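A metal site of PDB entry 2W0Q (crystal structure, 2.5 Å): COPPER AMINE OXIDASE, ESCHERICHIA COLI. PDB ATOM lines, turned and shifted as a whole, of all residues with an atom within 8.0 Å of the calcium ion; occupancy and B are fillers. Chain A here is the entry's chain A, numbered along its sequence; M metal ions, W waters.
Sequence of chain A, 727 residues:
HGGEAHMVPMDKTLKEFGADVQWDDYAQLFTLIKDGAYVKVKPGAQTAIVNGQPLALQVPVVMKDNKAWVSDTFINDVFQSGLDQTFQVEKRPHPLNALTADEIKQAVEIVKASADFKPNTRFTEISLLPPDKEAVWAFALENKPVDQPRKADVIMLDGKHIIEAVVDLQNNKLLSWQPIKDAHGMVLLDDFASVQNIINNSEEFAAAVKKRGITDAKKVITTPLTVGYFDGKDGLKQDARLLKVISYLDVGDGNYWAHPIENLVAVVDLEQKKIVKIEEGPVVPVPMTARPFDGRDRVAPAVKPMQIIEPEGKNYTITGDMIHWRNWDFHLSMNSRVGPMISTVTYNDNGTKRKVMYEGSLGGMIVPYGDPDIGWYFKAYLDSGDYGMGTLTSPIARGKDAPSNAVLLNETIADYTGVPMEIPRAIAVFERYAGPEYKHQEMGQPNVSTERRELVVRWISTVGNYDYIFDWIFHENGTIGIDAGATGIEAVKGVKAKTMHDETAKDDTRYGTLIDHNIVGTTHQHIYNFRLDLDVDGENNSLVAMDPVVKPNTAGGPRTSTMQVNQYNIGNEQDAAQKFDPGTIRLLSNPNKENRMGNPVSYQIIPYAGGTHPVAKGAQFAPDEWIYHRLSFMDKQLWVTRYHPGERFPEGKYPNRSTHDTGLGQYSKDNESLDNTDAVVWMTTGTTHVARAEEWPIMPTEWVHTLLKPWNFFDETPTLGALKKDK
The calcium ion is bound by water W1 (2.2 Å), O of Tyr 667 (2.5 Å), water W3 (2.6 Å), OE2 of Glu 573 (2.6 Å) and OE1 of Glu 672 (2.8 Å).
The calcium ion has five donor atoms within binding distance.
Residues that only touch the calcium ion: Glu 647 (3.99 Å).
Four residues have an atom within 4 Å of the calcium ion: Glu 573, Glu 647, Tyr 667 and Glu 672.
The side-chain carboxylate (OE2) of Glu 573 lies close to the backbone NH (N) of Arg 642 (3.0 Å).
The backbone NH of Glu 573 sits close to the side-chain amide nitrogen of Asn 671 (3.2 Å).
Water W1 lies within hydrogen-bond range of the backbone carbonyl oxygen of Arg 642 (2.5 Å) and the side-chain carboxylate of Glu 647 (2.6 Å).
Water W4 bridges the side-chain carboxylate of Glu 573 and the backbone NH of Asp 670.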
ATOM      1  N   GLU A 573       0.170   1.660  23.923  1.00  0.00           N
ATOM      2  CA  GLU A 573       0.064   1.397  22.495  1.00  0.00           C
ATOM      3  C   GLU A 573      -0.223   2.599  21.592  1.00  0.00           C
ATOM      4  O   GLU A 573       0.359   2.649  20.508  1.00  0.00           O
ATOM      5  CB  GLU A 573      -0.954   0.287  22.233  1.00  0.00           C
ATOM      6  CG  GLU A 573      -0.477  -1.110  22.714  1.00  0.00           C
ATOM      7  CD  GLU A 573      -1.584  -2.197  22.616  1.00  0.00           C
ATOM      8  OE1 GLU A 573      -2.805  -1.920  22.839  1.00  0.00           O
ATOM      9  OE2 GLU A 573      -1.229  -3.376  22.324  1.00  0.00           O
ATOM     10  N   VAL A 640       3.953  -0.638  18.418  1.00  0.00           N
ATOM     11  CA  VAL A 640       4.324  -1.589  19.442  1.00  0.00           C
ATOM     12  C   VAL A 640       3.023  -2.001  20.165  1.00  0.00           C
ATOM     13  O   VAL A 640       2.251  -1.133  20.668  1.00  0.00           O
ATOM     14  CB  VAL A 640       5.400  -1.068  20.430  1.00  0.00           C
ATOM     15  CG1 VAL A 640       5.811  -2.158  21.408  1.00  0.00           C
ATOM     16  CG2 VAL A 640       6.642  -0.516  19.695  1.00  0.00           C
ATOM     17  N   THR A 641       2.769  -3.307  20.166  1.00  0.00           N
ATOM     18  CA  THR A 641       1.558  -3.858  20.713  1.00  0.00           C
ATOM     19  C   THR A 641       1.949  -4.988  21.647  1.00  0.00           C
ATOM     20  O   THR A 641       3.079  -5.511  21.575  1.00  0.00           O
ATOM     21  CB  THR A 641       0.645  -4.381  19.576  1.00  0.00           C
ATOM     22  OG1 THR A 641       1.388  -5.280  18.742  1.00  0.00           O
ATOM     23  CG2 THR A 641       0.110  -3.227  18.712  1.00  0.00           C
ATOM     24  N   ARG A 642       1.022  -5.367  22.533  1.00  0.00           N
ATOM     25  CA  ARG A 642       1.281  -6.502  23.446  1.00  0.00           C
ATOM     26  C   ARG A 642       1.188  -7.776  22.642  1.00  0.00           C
ATOM     27  O   ARG A 642       0.300  -7.874  21.778  1.00  0.00           O
ATOM     28  CB  ARG A 642       0.279  -6.553  24.594  1.00  0.00           C
ATOM     29  CG  ARG A 642       0.445  -5.427  25.552  1.00  0.00           C
ATOM     30  CD  ARG A 642      -0.689  -5.375  26.541  1.00  0.00           C
ATOM     31  NE  ARG A 642      -0.600  -6.444  27.533  1.00  0.00           N
ATOM     32  CZ  ARG A 642      -0.007  -6.286  28.702  1.00  0.00           C
ATOM     33  NH1 ARG A 642       0.543  -5.126  29.016  1.00  0.00           N
ATOM     34  NH2 ARG A 642       0.029  -7.308  29.557  1.00  0.00           N
ATOM     35  N   TYR A 643       2.123  -8.688  22.912  1.00  0.00           N
ATOM     36  CA  TYR A 643       2.165  -9.952  22.233  1.00  0.00           C
ATOM     37  C   TYR A 643       0.838 -10.651  22.262  1.00  0.00           C
ATOM     38  O   TYR A 643       0.211 -10.727  23.318  1.00  0.00           O
ATOM     39  CB  TYR A 643       3.166 -10.871  22.896  1.00  0.00           C
ATOM     40  CG  TYR A 643       3.077 -12.272  22.331  1.00  0.00           C
ATOM     41  CD1 TYR A 643       3.518 -12.545  21.032  1.00  0.00           C
ATOM     42  CD2 TYR A 643       2.536 -13.346  23.081  1.00  0.00           C
ATOM     43  CE1 TYR A 643       3.425 -13.812  20.489  1.00  0.00           C
ATOM     44  CE2 TYR A 643       2.459 -14.614  22.572  1.00  0.00           C
ATOM     45  CZ  TYR A 643       2.911 -14.853  21.269  1.00  0.00           C
ATOM     46  OH  TYR A 643       2.847 -16.131  20.722  1.00  0.00           O
ATOM     47  N   HIS A 644       0.403 -11.183  21.127  1.00  0.00           N
ATOM     48  CA  HIS A 644      -0.813 -11.955  21.047  1.00  0.00           C
ATOM     49  C   HIS A 644      -0.716 -12.968  19.892  1.00  0.00           C
ATOM     50  O   HIS A 644      -0.590 -12.556  18.739  1.00  0.00           O
ATOM     51  CB  HIS A 644      -2.009 -11.036  20.810  1.00  0.00           C
ATOM     52  CG  HIS A 644      -3.305 -11.764  20.825  1.00  0.00           C
ATOM     53  ND1 HIS A 644      -4.452 -11.255  21.417  1.00  0.00           N
ATOM     54  CD2 HIS A 644      -3.642 -12.996  20.364  1.00  0.00           C
ATOM     55  CE1 HIS A 644      -5.435 -12.134  21.285  1.00  0.00           C
ATOM     56  NE2 HIS A 644      -4.962 -13.197  20.655  1.00  0.00           N
ATOM     57  N   GLU A 647      -2.505 -11.998  16.540  1.00  0.00           N
ATOM     58  CA  GLU A 647      -2.392 -10.728  15.829  1.00  0.00           C
ATOM     59  C   GLU A 647      -1.110 -10.775  14.986  1.00  0.00           C
ATOM     60  O   GLU A 647       0.030 -10.661  15.504  1.00  0.00           O
ATOM     61  CB  GLU A 647      -2.428  -9.535  16.775  1.00  0.00           C
ATOM     62  CG  GLU A 647      -3.697  -9.488  17.631  1.00  0.00           C
ATOM     63  CD  GLU A 647      -3.707  -8.341  18.668  1.00  0.00           C
ATOM     64  OE1 GLU A 647      -2.605  -7.811  19.045  1.00  0.00           O
ATOM     65  OE2 GLU A 647      -4.840  -7.971  19.078  1.00  0.00           O
ATOM     66  N   LEU A 664      -3.602  -3.449  12.526  1.00  0.00           N
ATOM     67  CA  LEU A 664      -2.913  -2.737  13.553  1.00  0.00           C
ATOM     68  C   LEU A 664      -3.777  -1.673  14.217  1.00  0.00           C
ATOM     69  O   LEU A 664      -3.557  -1.391  15.381  1.00  0.00           O
ATOM     70  CB  LEU A 664      -1.608  -2.139  13.024  1.00  0.00           C
ATOM     71  CG  LEU A 664      -0.393  -3.058  13.061  1.00  0.00           C
ATOM     72  CD1 LEU A 664       0.730  -2.478  12.232  1.00  0.00           C
ATOM     73  CD2 LEU A 664       0.047  -3.228  14.470  1.00  0.00           C
ATOM     74  N   GLN A 666      -6.953  -2.127  14.941  1.00  0.00           N
ATOM     75  CA  GLN A 666      -7.632  -2.931  15.954  1.00  0.00           C
ATOM     76  C   GLN A 666      -6.687  -3.408  17.060  1.00  0.00           C
ATOM     77  O   GLN A 666      -7.025  -3.292  18.252  1.00  0.00           O
ATOM     78  CB  GLN A 666      -8.314  -4.136  15.306  1.00  0.00           C
ATOM     79  CG  GLN A 666      -8.831  -5.207  16.238  1.00  0.00           C
ATOM     80  CD  GLN A 666      -9.389  -6.420  15.483  1.00  0.00           C
ATOM     81  OE1 GLN A 666     -10.276  -6.280  14.625  1.00  0.00           O
ATOM     82  NE2 GLN A 666      -8.859  -7.600  15.761  1.00  0.00           N
ATOM     83  N   TYR A 667      -5.513  -3.925  16.713  1.00  0.00           N
ATOM     84  CA  TYR A 667      -4.608  -4.454  17.722  1.00  0.00           C
ATOM     85  C   TYR A 667      -4.184  -3.373  18.740  1.00  0.00           C
ATOM     86  O   TYR A 667      -3.793  -3.699  19.844  1.00  0.00           O
ATOM     87  CB  TYR A 667      -3.350  -5.070  17.129  1.00  0.00           C
ATOM     88  CG  TYR A 667      -3.533  -6.030  15.984  1.00  0.00           C
ATOM     89  CD1 TYR A 667      -4.718  -6.739  15.804  1.00  0.00           C
ATOM     90  CD2 TYR A 667      -2.473  -6.269  15.109  1.00  0.00           C
ATOM     91  CE1 TYR A 667      -4.877  -7.630  14.740  1.00  0.00           C
ATOM     92  CE2 TYR A 667      -2.614  -7.167  14.043  1.00  0.00           C
ATOM     93  CZ  TYR A 667      -3.806  -7.839  13.869  1.00  0.00           C
ATOM     94  OH  TYR A 667      -3.923  -8.708  12.819  1.00  0.00           O
ATOM     95  N   SER A 668      -4.256  -2.110  18.374  1.00  0.00           N
ATOM     96  CA  SER A 668      -3.892  -1.042  19.281  1.00  0.00           C
ATOM     97  C   SER A 668      -5.097  -0.316  19.899  1.00  0.00           C
ATOM     98  O   SER A 668      -4.903   0.589  20.681  1.00  0.00           O
ATOM     99  CB  SER A 668      -2.971  -0.051  18.568  1.00  0.00           C
ATOM    100  OG  SER A 668      -3.631   0.614  17.495  1.00  0.00           O
ATOM    101  N   LYS A 669      -6.329  -0.719  19.567  1.00  0.00           N
ATOM    102  CA  LYS A 669      -7.565   0.044  19.910  1.00  0.00           C
ATOM    103  C   LYS A 669      -7.681   0.382  21.397  1.00  0.00           C
ATOM    104  O   LYS A 669      -8.004   1.502  21.773  1.00  0.00           O
ATOM    105  CB  LYS A 669      -8.840  -0.719  19.495  1.00  0.00           C
ATOM    106  CG  LYS A 669      -9.853   0.107  18.650  1.00  0.00           C
ATOM    107  CD  LYS A 669     -11.361   0.118  19.148  1.00  0.00           C
ATOM    108  CE  LYS A 669     -11.860  -1.209  19.841  1.00  0.00           C
ATOM    109  NZ  LYS A 669     -11.274  -2.487  19.278  1.00  0.00           N
ATOM    110  N   ASP A 670      -7.386  -0.600  22.243  1.00  0.00           N
ATOM    111  CA  ASP A 670      -7.624  -0.466  23.686  1.00  0.00           C
ATOM    112  C   ASP A 670      -6.459   0.130  24.392  1.00  0.00           C
ATOM    113  O   ASP A 670      -6.442   0.157  25.606  1.00  0.00           O
ATOM    114  CB  ASP A 670      -7.942  -1.834  24.313  1.00  0.00           C
ATOM    115  CG  ASP A 670      -9.204  -2.451  23.747  1.00  0.00           C
ATOM    116  OD1 ASP A 670     -10.220  -1.733  23.566  1.00  0.00           O
ATOM    117  OD2 ASP A 670      -9.169  -3.658  23.467  1.00  0.00           O
ATOM    118  N   ASN A 671      -5.465   0.586  23.650  1.00  0.00           N
ATOM    119  CA  ASN A 671      -4.358   1.334  24.227  1.00  0.00           C
ATOM    120  C   ASN A 671      -3.694   0.707  25.476  1.00  0.00           C
ATOM    121  O   ASN A 671      -3.552   1.344  26.534  1.00  0.00           O
ATOM    122  CB  ASN A 671      -4.819   2.755  24.511  1.00  0.00           C
ATOM    123  CG  ASN A 671      -3.680   3.707  24.655  1.00  0.00           C
ATOM    124  OD1 ASN A 671      -3.812   4.742  25.269  1.00  0.00           O
ATOM    125  ND2 ASN A 671      -2.547   3.359  24.088  1.00  0.00           N
ATOM    126  N   GLU A 672      -3.270  -0.543  25.355  1.00  0.00           N
ATOM    127  CA  GLU A 672      -2.795  -1.254  26.527  1.00  0.00           C
ATOM    128  C   GLU A 672      -1.390  -0.856  26.980  1.00  0.00           C
ATOM    129  O   GLU A 672      -0.608  -0.219  26.249  1.00  0.00           O
ATOM    130  CB  GLU A 672      -2.901  -2.757  26.303  1.00  0.00           C
ATOM    131  CG  GLU A 672      -4.260  -3.192  25.722  1.00  0.00           C
ATOM    132  CD  GLU A 672      -4.396  -4.721  25.594  1.00  0.00           C
ATOM    133  OE1 GLU A 672      -4.182  -5.267  24.469  1.00  0.00           O
ATOM    134  OE2 GLU A 672      -4.704  -5.387  26.620  1.00  0.00           O
ATOM    135  N   SER A 673      -1.085  -1.226  28.214  1.00  0.00           N
ATOM    136  CA  SER A 673       0.179  -0.908  28.797  1.00  0.00           C
ATOM    137  C   SER A 673       1.292  -1.644  28.067  1.00  0.00           C
ATOM    138  O   SER A 673       1.152  -2.808  27.708  1.00  0.00           O
ATOM    139  CB  SER A 673       0.212  -1.284  30.280  1.00  0.00           C
ATOM    140  OG  SER A 673       1.525  -1.046  30.792  1.00  0.00           O
ATOM    141  N   LEU A 674       2.409  -0.934  27.863  1.00  0.00           N
ATOM    142  CA  LEU A 674       3.589  -1.531  27.275  1.00  0.00           C
ATOM    143  C   LEU A 674       4.706  -1.496  28.279  1.00  0.00           C
ATOM    144  O   LEU A 674       5.866  -1.481  27.918  1.00  0.00           O
ATOM    145  CB  LEU A 674       3.990  -0.796  26.021  1.00  0.00           C
ATOM    146  CG  LEU A 674       3.083  -1.042  24.811  1.00  0.00           C
ATOM    147  CD1 LEU A 674       3.430  -0.015  23.757  1.00  0.00           C
ATOM    148  CD2 LEU A 674       3.227  -2.485  24.273  1.00  0.00           C
HETATM  149 CA    CA M   1      -3.157  -5.051  21.870  1.00  0.00          CA
HETATM  150  O   HOH W   1      -2.067  -6.977  21.470  1.00  0.00           O
HETATM  151  O   HOH W   2      -4.142  -7.978  23.376  1.00  0.00           O
HETATM  152  O   HOH W   3      -5.109  -6.563  21.082  1.00  0.00           O
HETATM  153  O   HOH W   4      -5.374  -2.858  22.325  1.00  0.00           O
